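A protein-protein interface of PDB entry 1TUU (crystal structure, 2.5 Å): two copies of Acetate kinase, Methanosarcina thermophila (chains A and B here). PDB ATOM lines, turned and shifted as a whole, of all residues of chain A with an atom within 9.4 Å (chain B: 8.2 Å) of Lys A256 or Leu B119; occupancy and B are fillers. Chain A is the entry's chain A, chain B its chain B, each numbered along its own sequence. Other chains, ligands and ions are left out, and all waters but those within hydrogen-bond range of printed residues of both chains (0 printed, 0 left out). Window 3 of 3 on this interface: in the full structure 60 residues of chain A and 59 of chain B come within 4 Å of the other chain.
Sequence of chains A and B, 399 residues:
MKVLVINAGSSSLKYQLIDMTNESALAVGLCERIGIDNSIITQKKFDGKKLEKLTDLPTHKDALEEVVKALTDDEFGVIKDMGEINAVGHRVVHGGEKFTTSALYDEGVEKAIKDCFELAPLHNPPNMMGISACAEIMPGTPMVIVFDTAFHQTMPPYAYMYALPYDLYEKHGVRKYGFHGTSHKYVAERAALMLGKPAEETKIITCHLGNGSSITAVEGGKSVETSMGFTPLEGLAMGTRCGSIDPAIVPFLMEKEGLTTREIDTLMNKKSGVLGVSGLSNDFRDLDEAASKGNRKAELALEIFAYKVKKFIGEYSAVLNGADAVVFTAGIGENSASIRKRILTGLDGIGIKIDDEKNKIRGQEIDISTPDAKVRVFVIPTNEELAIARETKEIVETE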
ATOM      1  N   ALA A 248      -3.384 -14.318  21.210  1.00  0.00           N
ATOM      2  CA  ALA A 248      -2.253 -13.920  20.403  1.00  0.00           C
ATOM      3  C   ALA A 248      -2.258 -14.656  19.059  1.00  0.00           C
ATOM      4  O   ALA A 248      -1.633 -14.194  18.103  1.00  0.00           O
ATOM      5  CB  ALA A 248      -0.947 -14.196  21.162  1.00  0.00           C
ATOM      6  N   ILE A 249      -2.970 -15.786  18.981  1.00  0.00           N
ATOM      7  CA  ILE A 249      -3.044 -16.568  17.740  1.00  0.00           C
ATOM      8  C   ILE A 249      -3.774 -15.815  16.631  1.00  0.00           C
ATOM      9  O   ILE A 249      -3.501 -16.008  15.446  1.00  0.00           O
ATOM     10  CB  ILE A 249      -3.747 -17.925  17.956  1.00  0.00           C
ATOM     11  CG1 ILE A 249      -2.919 -18.769  18.913  1.00  0.00           C
ATOM     12  CG2 ILE A 249      -3.887 -18.682  16.642  1.00  0.00           C
ATOM     13  CD1 ILE A 249      -3.498 -20.137  19.153  1.00  0.00           C
ATOM     14  N   VAL A 250      -4.712 -14.963  17.020  1.00  0.00           N
ATOM     15  CA  VAL A 250      -5.457 -14.167  16.060  1.00  0.00           C
ATOM     16  C   VAL A 250      -4.505 -13.287  15.244  1.00  0.00           C
ATOM     17  O   VAL A 250      -4.368 -13.464  14.026  1.00  0.00           O
ATOM     18  CB  VAL A 250      -6.464 -13.281  16.772  1.00  0.00           C
ATOM     19  CG1 VAL A 250      -7.317 -12.558  15.757  1.00  0.00           C
ATOM     20  CG2 VAL A 250      -7.320 -14.122  17.697  1.00  0.00           C
ATOM     21  N   PRO A 251      -3.818 -12.335  15.908  1.00  0.00           N
ATOM     22  CA  PRO A 251      -2.897 -11.472  15.158  1.00  0.00           C
ATOM     23  C   PRO A 251      -1.844 -12.298  14.415  1.00  0.00           C
ATOM     24  O   PRO A 251      -1.467 -11.975  13.283  1.00  0.00           O
ATOM     25  CB  PRO A 251      -2.297 -10.583  16.244  1.00  0.00           C
ATOM     26  CG  PRO A 251      -2.251 -11.487  17.412  1.00  0.00           C
ATOM     27  CD  PRO A 251      -3.607 -12.179  17.358  1.00  0.00           C
ATOM     28  N   PHE A 252      -1.384 -13.369  15.059  1.00  0.00           N
ATOM     29  CA  PHE A 252      -0.389 -14.251  14.462  1.00  0.00           C
ATOM     30  C   PHE A 252      -0.889 -14.827  13.142  1.00  0.00           C
ATOM     31  O   PHE A 252      -0.254 -14.667  12.094  1.00  0.00           O
ATOM     32  CB  PHE A 252      -0.079 -15.408  15.404  1.00  0.00           C
ATOM     33  CG  PHE A 252       0.771 -16.478  14.789  1.00  0.00           C
ATOM     34  CD1 PHE A 252       2.144 -16.306  14.663  1.00  0.00           C
ATOM     35  CD2 PHE A 252       0.203 -17.679  14.369  1.00  0.00           C
ATOM     36  CE1 PHE A 252       2.947 -17.314  14.134  1.00  0.00           C
ATOM     37  CE2 PHE A 252       0.996 -18.694  13.839  1.00  0.00           C
ATOM     38  CZ  PHE A 252       2.370 -18.512  13.723  1.00  0.00           C
ATOM     39  N   LEU A 253      -2.031 -15.502  13.211  1.00  0.00           N
ATOM     40  CA  LEU A 253      -2.634 -16.129  12.053  1.00  0.00           C
ATOM     41  C   LEU A 253      -2.982 -15.096  10.994  1.00  0.00           C
ATOM     42  O   LEU A 253      -3.047 -15.412   9.811  1.00  0.00           O
ATOM     43  CB  LEU A 253      -3.899 -16.883  12.469  1.00  0.00           C
ATOM     44  CG  LEU A 253      -4.094 -18.226  11.776  1.00  0.00           C
ATOM     45  CD1 LEU A 253      -2.871 -19.102  12.036  1.00  0.00           C
ATOM     46  CD2 LEU A 253      -5.358 -18.902  12.297  1.00  0.00           C
ATOM     47  N   MET A 254      -3.222 -13.864  11.425  1.00  0.00           N
ATOM     48  CA  MET A 254      -3.562 -12.792  10.502  1.00  0.00           C
ATOM     49  C   MET A 254      -2.332 -12.384   9.687  1.00  0.00           C
ATOM     50  O   MET A 254      -2.420 -12.181   8.481  1.00  0.00           O
ATOM     51  CB  MET A 254      -4.129 -11.593  11.274  1.00  0.00           C
ATOM     52  CG  MET A 254      -5.587 -11.781  11.706  1.00  0.00           C
ATOM     53  SD  MET A 254      -6.275 -10.436  12.702  1.00  0.00           S
ATOM     54  CE  MET A 254      -6.953  -9.387  11.452  1.00  0.00           C
ATOM     55  N   GLU A 255      -1.184 -12.290  10.352  1.00  0.00           N
ATOM     56  CA  GLU A 255       0.069 -11.929   9.699  1.00  0.00           C
ATOM     57  C   GLU A 255       0.595 -13.065   8.830  1.00  0.00           C
ATOM     58  O   GLU A 255       1.003 -12.849   7.692  1.00  0.00           O
ATOM     59  CB  GLU A 255       1.127 -11.574  10.744  1.00  0.00           C
ATOM     60  CG  GLU A 255       0.741 -10.412  11.631  1.00  0.00           C
ATOM     61  CD  GLU A 255       1.865  -9.991  12.554  1.00  0.00           C
ATOM     62  OE1 GLU A 255       2.948  -9.617  12.045  1.00  0.00           O
ATOM     63  OE2 GLU A 255       1.669 -10.028  13.790  1.00  0.00           O
ATOM     64  N   LYS A 256       0.593 -14.280   9.363  1.00  0.00           N
ATOM     65  CA  LYS A 256       1.088 -15.420   8.608  1.00  0.00           C
ATOM     66  C   LYS A 256       0.264 -15.743   7.372  1.00  0.00           C
ATOM     67  O   LYS A 256       0.822 -16.066   6.325  1.00  0.00           O
ATOM     68  CB  LYS A 256       1.160 -16.658   9.506  1.00  0.00           C
ATOM     69  CG  LYS A 256       2.473 -16.805  10.249  1.00  0.00           C
ATOM     70  CD  LYS A 256       3.555 -17.382   9.345  1.00  0.00           C
ATOM     71  CE  LYS A 256       4.865 -17.569  10.112  1.00  0.00           C
ATOM     72  NZ  LYS A 256       5.848 -18.425   9.374  1.00  0.00           N
ATOM     73  N   GLU A 257      -1.058 -15.669   7.487  1.00  0.00           N
ATOM     74  CA  GLU A 257      -1.933 -15.972   6.360  1.00  0.00           C
ATOM     75  C   GLU A 257      -2.473 -14.700   5.697  1.00  0.00           C
ATOM     76  O   GLU A 257      -3.167 -14.772   4.692  1.00  0.00           O
ATOM     77  CB  GLU A 257      -3.104 -16.854   6.824  1.00  0.00           C
ATOM     78  CG  GLU A 257      -2.689 -18.072   7.665  1.00  0.00           C
ATOM     79  CD  GLU A 257      -2.322 -19.298   6.832  1.00  0.00           C
ATOM     80  OE1 GLU A 257      -1.520 -19.163   5.879  1.00  0.00           O
ATOM     81  OE2 GLU A 257      -2.824 -20.401   7.136  1.00  0.00           O
ATOM     82  N   GLY A 258      -2.152 -13.543   6.263  1.00  0.00           N
ATOM     83  CA  GLY A 258      -2.629 -12.302   5.691  1.00  0.00           C
ATOM     84  C   GLY A 258      -4.141 -12.287   5.619  1.00  0.00           C
ATOM     85  O   GLY A 258      -4.725 -11.828   4.640  1.00  0.00           O
ATOM     86  N   LEU A 259      -4.779 -12.805   6.662  1.00  0.00           N
ATOM     87  CA  LEU A 259      -6.233 -12.854   6.723  1.00  0.00           C
ATOM     88  C   LEU A 259      -6.808 -11.555   7.267  1.00  0.00           C
ATOM     89  O   LEU A 259      -6.171 -10.873   8.062  1.00  0.00           O
ATOM     90  CB  LEU A 259      -6.675 -14.007   7.609  1.00  0.00           C
ATOM     91  CG  LEU A 259      -6.045 -15.353   7.289  1.00  0.00           C
ATOM     92  CD1 LEU A 259      -6.720 -16.399   8.156  1.00  0.00           C
ATOM     93  CD2 LEU A 259      -6.204 -15.705   5.822  1.00  0.00           C
ATOM     94  N   ILE A 264     -10.703 -14.052   9.746  1.00  0.00           N
ATOM     95  CA  ILE A 264     -10.271 -14.739  10.959  1.00  0.00           C
ATOM     96  C   ILE A 264     -11.483 -15.046  11.828  1.00  0.00           C
ATOM     97  O   ILE A 264     -11.481 -15.989  12.614  1.00  0.00           O
ATOM     98  CB  ILE A 264      -9.241 -13.897  11.771  1.00  0.00           C
ATOM     99  CG1 ILE A 264      -8.463 -14.789  12.741  1.00  0.00           C
ATOM    100  CG2 ILE A 264      -9.956 -12.866  12.622  1.00  0.00           C
ATOM    101  CD1 ILE A 264      -7.573 -15.827  12.095  1.00  0.00           C
ATOM    102  N   HIS B  94      12.011 -19.122  25.178  1.00  0.00           N
ATOM    103  CA  HIS B  94      11.340 -19.872  24.124  1.00  0.00           C
ATOM    104  C   HIS B  94      12.097 -21.115  23.633  1.00  0.00           C
ATOM    105  O   HIS B  94      13.183 -21.014  23.046  1.00  0.00           O
ATOM    106  CB  HIS B  94      11.037 -18.955  22.926  1.00  0.00           C
ATOM    107  CG  HIS B  94       9.953 -19.482  22.036  1.00  0.00           C
ATOM    108  ND1 HIS B  94      10.052 -20.687  21.372  1.00  0.00           N
ATOM    109  CD2 HIS B  94       8.728 -18.987  21.739  1.00  0.00           C
ATOM    110  CE1 HIS B  94       8.935 -20.912  20.704  1.00  0.00           C
ATOM    111  NE2 HIS B  94       8.116 -19.896  20.910  1.00  0.00           N
ATOM    112  N   GLY B  96      10.036 -23.757  22.243  1.00  0.00           N
ATOM    113  CA  GLY B  96       9.139 -24.333  21.259  1.00  0.00           C
ATOM    114  C   GLY B  96       9.137 -25.852  21.253  1.00  0.00           C
ATOM    115  O   GLY B  96       9.312 -26.495  22.288  1.00  0.00           O
ATOM    116  N   GLU B  97       8.907 -26.420  20.074  1.00  0.00           N
ATOM    117  CA  GLU B  97       8.889 -27.865  19.888  1.00  0.00           C
ATOM    118  C   GLU B  97      10.345 -28.320  19.808  1.00  0.00           C
ATOM    119  O   GLU B  97      11.238 -27.627  20.305  1.00  0.00           O
ATOM    120  CB  GLU B  97       8.129 -28.228  18.593  1.00  0.00           C
ATOM    121  CG  GLU B  97       6.593 -28.138  18.709  1.00  0.00           C
ATOM    122  CD  GLU B  97       5.862 -28.040  17.359  1.00  0.00           C
ATOM    123  OE1 GLU B  97       6.161 -27.106  16.580  1.00  0.00           O
ATOM    124  OE2 GLU B  97       4.983 -28.893  17.085  1.00  0.00           O
ATOM    125  N   LYS B 111      20.759 -23.781  15.527  1.00  0.00           N
ATOM    126  CA  LYS B 111      19.871 -23.581  14.377  1.00  0.00           C
ATOM    127  C   LYS B 111      18.414 -23.393  14.823  1.00  0.00           C
ATOM    128  O   LYS B 111      17.811 -22.347  14.568  1.00  0.00           O
ATOM    129  CB  LYS B 111      19.966 -24.781  13.412  1.00  0.00           C
ATOM    130  CG  LYS B 111      21.366 -25.060  12.878  1.00  0.00           C
ATOM    131  CD  LYS B 111      21.369 -26.070  11.721  1.00  0.00           C
ATOM    132  CE  LYS B 111      21.058 -27.500  12.165  1.00  0.00           C
ATOM    133  NZ  LYS B 111      19.648 -27.707  12.610  1.00  0.00           N
ATOM    134  N   ALA B 112      17.862 -24.406  15.491  1.00  0.00           N
ATOM    135  CA  ALA B 112      16.480 -24.359  15.971  1.00  0.00           C
ATOM    136  C   ALA B 112      16.173 -23.107  16.797  1.00  0.00           C
ATOM    137  O   ALA B 112      15.031 -22.642  16.826  1.00  0.00           O
ATOM    138  CB  ALA B 112      16.168 -25.613  16.789  1.00  0.00           C
ATOM    139  N   LYS B 114      17.599 -20.162  16.258  1.00  0.00           N
ATOM    140  CA  LYS B 114      17.556 -19.061  15.304  1.00  0.00           C
ATOM    141  C   LYS B 114      16.330 -19.229  14.396  1.00  0.00           C
ATOM    142  O   LYS B 114      15.693 -18.248  13.995  1.00  0.00           O
ATOM    143  CB  LYS B 114      18.849 -19.043  14.479  1.00  0.00           C
ATOM    144  CG  LYS B 114      20.125 -19.040  15.334  1.00  0.00           C
ATOM    145  CD  LYS B 114      21.416 -19.186  14.505  1.00  0.00           C
ATOM    146  CE  LYS B 114      21.613 -18.028  13.530  1.00  0.00           C
ATOM    147  NZ  LYS B 114      22.836 -18.206  12.688  1.00  0.00           N
ATOM    148  N   ASP B 115      16.006 -20.481  14.082  1.00  0.00           N
ATOM    149  CA  ASP B 115      14.856 -20.806  13.236  1.00  0.00           C
ATOM    150  C   ASP B 115      13.543 -20.308  13.839  1.00  0.00           C
ATOM    151  O   ASP B 115      12.693 -19.760  13.135  1.00  0.00           O
ATOM    152  CB  ASP B 115      14.764 -22.325  13.024  1.00  0.00           C
ATOM    153  CG  ASP B 115      15.665 -22.825  11.903  1.00  0.00           C
ATOM    154  OD1 ASP B 115      16.856 -22.451  11.871  1.00  0.00           O
ATOM    155  OD2 ASP B 115      15.174 -23.605  11.058  1.00  0.00           O
ATOM    156  N   CYS B 116      13.388 -20.492  15.147  1.00  0.00           N
ATOM    157  CA  CYS B 116      12.172 -20.088  15.847  1.00  0.00           C
ATOM    158  C   CYS B 116      12.070 -18.583  16.133  1.00  0.00           C
ATOM    159  O   CYS B 116      12.137 -18.152  17.285  1.00  0.00           O
ATOM    160  CB  CYS B 116      12.058 -20.890  17.154  1.00  0.00           C
ATOM    161  SG  CYS B 116      10.373 -21.112  17.819  1.00  0.00           S
ATOM    162  N   PHE B 117      11.926 -17.787  15.077  1.00  0.00           N
ATOM    163  CA  PHE B 117      11.781 -16.336  15.215  1.00  0.00           C
ATOM    164  C   PHE B 117      10.447 -15.882  14.617  1.00  0.00           C
ATOM    165  O   PHE B 117       9.617 -15.282  15.308  1.00  0.00           O
ATOM    166  CB  PHE B 117      12.931 -15.585  14.528  1.00  0.00           C
ATOM    167  CG  PHE B 117      14.207 -15.557  15.330  1.00  0.00           C
ATOM    168  CD1 PHE B 117      14.181 -15.719  16.716  1.00  0.00           C
ATOM    169  CD2 PHE B 117      15.434 -15.334  14.706  1.00  0.00           C
ATOM    170  CE1 PHE B 117      15.357 -15.663  17.465  1.00  0.00           C
ATOM    171  CE2 PHE B 117      16.617 -15.275  15.447  1.00  0.00           C
ATOM    172  CZ  PHE B 117      16.577 -15.440  16.828  1.00  0.00           C
ATOM    173  N   GLU B 118      10.246 -16.180  13.334  1.00  0.00           N
ATOM    174  CA  GLU B 118       9.010 -15.821  12.647  1.00  0.00           C
ATOM    175  C   GLU B 118       7.982 -16.942  12.808  1.00  0.00           C
ATOM    176  O   GLU B 118       6.808 -16.790  12.446  1.00  0.00           O
ATOM    177  CB  GLU B 118       9.296 -15.571  11.164  1.00  0.00           C
ATOM    178  CG  GLU B 118      10.048 -14.278  10.905  1.00  0.00           C
ATOM    179  CD  GLU B 118      11.303 -14.480  10.082  1.00  0.00           C
ATOM    180  OE1 GLU B 118      12.181 -15.255  10.523  1.00  0.00           O
ATOM    181  OE2 GLU B 118      11.407 -13.868   8.995  1.00  0.00           O
ATOM    182  N   LEU B 119       8.435 -18.065  13.362  1.00  0.00           N
ATOM    183  CA  LEU B 119       7.572 -19.220  13.584  1.00  0.00           C
ATOM    184  C   LEU B 119       6.916 -19.119  14.964  1.00  0.00           C
ATOM    185  O   LEU B 119       6.320 -20.079  15.459  1.00  0.00           O
ATOM    186  CB  LEU B 119       8.390 -20.514  13.480  1.00  0.00           C
ATOM    187  CG  LEU B 119       9.415 -20.605  12.342  1.00  0.00           C
ATOM    188  CD1 LEU B 119      10.018 -22.005  12.349  1.00  0.00           C
ATOM    189  CD2 LEU B 119       8.773 -20.307  10.994  1.00  0.00           C
ATOM    190  N   ALA B 120       7.041 -17.946  15.581  1.00  0.00           N
ATOM    191  CA  ALA B 120       6.466 -17.686  16.897  1.00  0.00           C
ATOM    192  C   ALA B 120       6.411 -16.178  17.118  1.00  0.00           C
ATOM    193  O   ALA B 120       7.332 -15.444  16.738  1.00  0.00           O
ATOM    194  CB  ALA B 120       7.303 -18.352  17.984  1.00  0.00           C
ATOM    195  N   PRO B 121       5.321 -15.689  17.728  1.00  0.00           N
ATOM    196  CA  PRO B 121       5.132 -14.258  18.003  1.00  0.00           C
ATOM    197  C   PRO B 121       5.620 -13.802  19.387  1.00  0.00           C
ATOM    198  O   PRO B 121       4.894 -13.103  20.107  1.00  0.00           O
ATOM    199  CB  PRO B 121       3.629 -14.092  17.841  1.00  0.00           C
ATOM    200  CG  PRO B 121       3.123 -15.348  18.477  1.00  0.00           C
ATOM    201  CD  PRO B 121       4.073 -16.436  17.966  1.00  0.00           C
ATOM    202  N   LEU B 122       6.842 -14.203  19.753  1.00  0.00           N
ATOM    203  CA  LEU B 122       7.434 -13.828  21.043  1.00  0.00           C
ATOM    204  C   LEU B 122       8.104 -12.462  20.893  1.00  0.00           C
ATOM    205  O   LEU B 122       8.555 -12.099  19.798  1.00  0.00           O
ATOM    206  CB  LEU B 122       8.455 -14.885  21.502  1.00  0.00           C
ATOM    207  CG  LEU B 122       9.086 -14.704  22.898  1.00  0.00           C
ATOM    208  CD1 LEU B 122       7.998 -14.439  23.936  1.00  0.00           C
ATOM    209  CD2 LEU B 122       9.892 -15.958  23.271  1.00  0.00           C
ATOM    210  N   LEU B 168      -3.305 -25.832  10.790  1.00  0.00           N
ATOM    211  CA  LEU B 168      -2.553 -24.784  11.485  1.00  0.00           C
ATOM    212  C   LEU B 168      -1.448 -25.374  12.359  1.00  0.00           C
ATOM    213  O   LEU B 168      -0.345 -24.836  12.436  1.00  0.00           O
ATOM    214  CB  LEU B 168      -3.496 -23.920  12.336  1.00  0.00           C
ATOM    215  CG  LEU B 168      -4.613 -23.152  11.598  1.00  0.00           C
ATOM    216  CD1 LEU B 168      -5.504 -22.410  12.598  1.00  0.00           C
ATOM    217  CD2 LEU B 168      -3.991 -22.167  10.619  1.00  0.00           C
ATOM    218  N   LYS B 171       1.157 -27.131   9.727  1.00  0.00           N
ATOM    219  CA  LYS B 171       1.951 -26.284   8.851  1.00  0.00           C
ATOM    220  C   LYS B 171       2.467 -24.987   9.477  1.00  0.00           C
ATOM    221  O   LYS B 171       3.311 -24.309   8.893  1.00  0.00           O
ATOM    222  CB  LYS B 171       1.157 -25.974   7.573  1.00  0.00           C
ATOM    223  CG  LYS B 171       1.992 -25.336   6.494  1.00  0.00           C
ATOM    224  CD  LYS B 171       1.156 -24.828   5.324  1.00  0.00           C
ATOM    225  CE  LYS B 171       1.986 -23.900   4.430  1.00  0.00           C
ATOM    226  NZ  LYS B 171       2.569 -22.745   5.202  1.00  0.00           N
ATOM    227  N   HIS B 172       1.982 -24.645  10.668  1.00  0.00           N
ATOM    228  CA  HIS B 172       2.421 -23.421  11.343  1.00  0.00           C
ATOM    229  C   HIS B 172       2.812 -23.655  12.802  1.00  0.00           C
ATOM    230  O   HIS B 172       3.189 -22.721  13.502  1.00  0.00           O
ATOM    231  CB  HIS B 172       1.326 -22.350  11.272  1.00  0.00           C
ATOM    232  CG  HIS B 172       1.047 -21.867   9.884  1.00  0.00           C
ATOM    233  ND1 HIS B 172       1.887 -21.003   9.212  1.00  0.00           N
ATOM    234  CD2 HIS B 172       0.029 -22.144   9.032  1.00  0.00           C
ATOM    235  CE1 HIS B 172       1.394 -20.768   8.008  1.00  0.00           C
ATOM    236  NE2 HIS B 172       0.268 -21.447   7.874  1.00  0.00           N
ATOM    237  N   GLY B 173       2.712 -24.899  13.259  1.00  0.00           N
ATOM    238  CA  GLY B 173       3.080 -25.220  14.626  1.00  0.00           C
ATOM    239  C   GLY B 173       2.191 -24.679  15.737  1.00  0.00           C
ATOM    240  O   GLY B 173       2.601 -24.662  16.899  1.00  0.00           O
ATOM    241  N   VAL B 174       0.975 -24.258  15.411  1.00  0.00           N
ATOM    242  CA  VAL B 174       0.072 -23.723  16.427  1.00  0.00           C
ATOM    243  C   VAL B 174      -0.387 -24.762  17.458  1.00  0.00           C
ATOM    244  O   VAL B 174      -1.216 -25.629  17.169  1.00  0.00           O
ATOM    245  CB  VAL B 174      -1.177 -23.077  15.779  1.00  0.00           C
ATOM    246  CG1 VAL B 174      -2.152 -22.621  16.857  1.00  0.00           C
ATOM    247  CG2 VAL B 174      -0.758 -21.902  14.904  1.00  0.00           C
ATOM    248  N   TYR B 177       2.422 -24.523  24.204  1.00  0.00           N
ATOM    249  CA  TYR B 177       3.794 -24.809  24.621  1.00  0.00           C
ATOM    250  C   TYR B 177       3.981 -24.614  26.123  1.00  0.00           C
ATOM    251  O   TYR B 177       4.570 -25.456  26.806  1.00  0.00           O
ATOM    252  CB  TYR B 177       4.791 -23.904  23.888  1.00  0.00           C
ATOM    253  CG  TYR B 177       4.942 -24.219  22.420  1.00  0.00           C
ATOM    254  CD1 TYR B 177       5.477 -25.435  22.001  1.00  0.00           C
ATOM    255  CD2 TYR B 177       4.505 -23.324  21.450  1.00  0.00           C
ATOM    256  CE1 TYR B 177       5.566 -25.761  20.660  1.00  0.00           C
ATOM    257  CE2 TYR B 177       4.587 -23.639  20.106  1.00  0.00           C
ATOM    258  CZ  TYR B 177       5.118 -24.864  19.715  1.00  0.00           C
ATOM    259  OH  TYR B 177       5.176 -25.212  18.384  1.00  0.00           O
ATOM    260  N   PHE B 230       0.340 -21.149  23.309  1.00  0.00           N
ATOM    261  CA  PHE B 230       1.139 -20.834  22.146  1.00  0.00           C
ATOM    262  C   PHE B 230       2.070 -19.669  22.502  1.00  0.00           C
ATOM    263  O   PHE B 230       3.210 -19.624  22.054  1.00  0.00           O
ATOM    264  CB  PHE B 230       0.204 -20.462  20.993  1.00  0.00           C
ATOM    265  CG  PHE B 230       0.902 -20.230  19.689  1.00  0.00           C
ATOM    266  CD1 PHE B 230       1.616 -21.250  19.067  1.00  0.00           C
ATOM    267  CD2 PHE B 230       0.831 -18.989  19.074  1.00  0.00           C
ATOM    268  CE1 PHE B 230       2.251 -21.027  17.846  1.00  0.00           C
ATOM    269  CE2 PHE B 230       1.460 -18.760  17.857  1.00  0.00           C
ATOM    270  CZ  PHE B 230       2.170 -19.775  17.242  1.00  0.00           C
ATOM    271  N   THR B 261      -2.314  -5.401  13.233  1.00  0.00           N
ATOM    272  CA  THR B 261      -2.062  -6.663  13.916  1.00  0.00           C
ATOM    273  C   THR B 261      -1.072  -6.411  15.043  1.00  0.00           C
ATOM    274  O   THR B 261      -1.320  -6.793  16.184  1.00  0.00           O
ATOM    275  CB  THR B 261      -1.499  -7.751  12.966  1.00  0.00           C
ATOM    276  OG1 THR B 261      -0.084  -7.587  12.805  1.00  0.00           O
ATOM    277  CG2 THR B 261      -2.167  -7.659  11.599  1.00  0.00           C
ATOM    278  N   ARG B 262       0.041  -5.748  14.738  1.00  0.00           N
ATOM    279  CA  ARG B 262       1.028  -5.480  15.772  1.00  0.00           C
ATOM    280  C   ARG B 262       0.473  -4.608  16.893  1.00  0.00           C
ATOM    281  O   ARG B 262       0.873  -4.741  18.046  1.00  0.00           O
ATOM    282  CB  ARG B 262       2.293  -4.849  15.175  1.00  0.00           C
ATOM    283  CG  ARG B 262       3.267  -5.875  14.556  1.00  0.00           C
ATOM    284  CD  ARG B 262       2.858  -6.342  13.153  1.00  0.00           C
ATOM    285  NE  ARG B 262       3.346  -5.446  12.098  1.00  0.00           N
ATOM    286  CZ  ARG B 262       3.005  -5.525  10.812  1.00  0.00           C
ATOM    287  NH1 ARG B 262       2.160  -6.464  10.401  1.00  0.00           N
ATOM    288  NH2 ARG B 262       3.506  -4.659   9.935  1.00  0.00           N
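The side-chain hydroxyl (OG1) of Thr B261 lies close to the side-chain carboxylate (OE2) of Glu A255 (3.2 Å). The side-chain carboxylate (OE2) of Glu A257 is in hydrogen-bond range of a ring nitrogen (NE2) of His B172 (3.3 Å). The side-chain carboxylate (OE1) of Glu A255 is in salt-bridge range of the guanidinium group (NH1) of Arg B262 (3.6 Å).
The backbone NH (N) of Val B174 lies within hydrogen-bond range of the backbone carbonyl oxygen (O) of Leu B168, 3.3 Å away. NH1 of Arg B262 lies close to OG1 of Thr B261 (3.5 Å). The backbone carbonyl oxygen (O) of Leu B168 sits at hydrogen-bond distance from the backbone NH (N) of Gly B173 (3.2 Å).
CG1 of Val B174 touches CD1 of Ile A249 (3.6 Å). Phe B230 touches Ile A249 (CD2 to CG1, 3.8 Å). Pro A251 touches Thr B261. Pro B121 touches Phe A252 (CD to CD1, 3.8 Å). CE2 of Phe A252 touches CG2 of Val B174 (3.8 Å). CZ of Phe B230 touches CZ of Phe A252, at 3.7 Å. CD2 of Leu A253 touches CD1 of Leu B168 (3.5 Å). CE of Lys A256 touches O of Glu B118 (3.1 Å). NZ of Lys A256 touches CD2 of Leu B119, 3.8 Å away. CD of Lys A256 touches ND1 of His B172 (3.99 Å).
Of the printed residues of chain B, Lys A256 touches Glu B118, Leu B119 and His B172. Of the printed residues of chain B, Glu A257 touches His B172 (3.3 Å). Of chain A, only Lys A256 (3.8 Å) comes within 4 Å of Leu B119. No residue of chain A comes within 4 Å of Ala B120. Of the printed residues of chain A, Phe B230 touches Ile A249 (3.8 Å) and Phe A252 (3.7 Å). Printed residues of chain A within 4 Å of Thr B261: Pro A251 and Glu A255. The nearest printed residue of chain B that does not touch Lys A256 is Ala B120 (5.9 Å).
Of the 13 printed residues of chain A, 7 touch a printed residue of chain B. Hydrophobic or aromatic side chains of chain A that line the printed part of chain B: Ile A249, Pro A251, Phe A252 and Leu A253. Hydrophobic or aromatic side chains of chain B within 4 Å of the printed part of chain A: Leu B119, Pro B121, Leu B168, His B172, Val B174 and Phe B230. Among the printed residues, 13 pairs touch across the chains. Among the printed residues, Asp or Glu carboxylates within 4 Å of a Lys or Arg side-chain nitrogen of the other chain: Glu A255 with Arg B262.
No position is printed for both chains. Of the 13 pairs that touch across the chains among the printed residues, none has its exchanged pair printed and touching as well.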
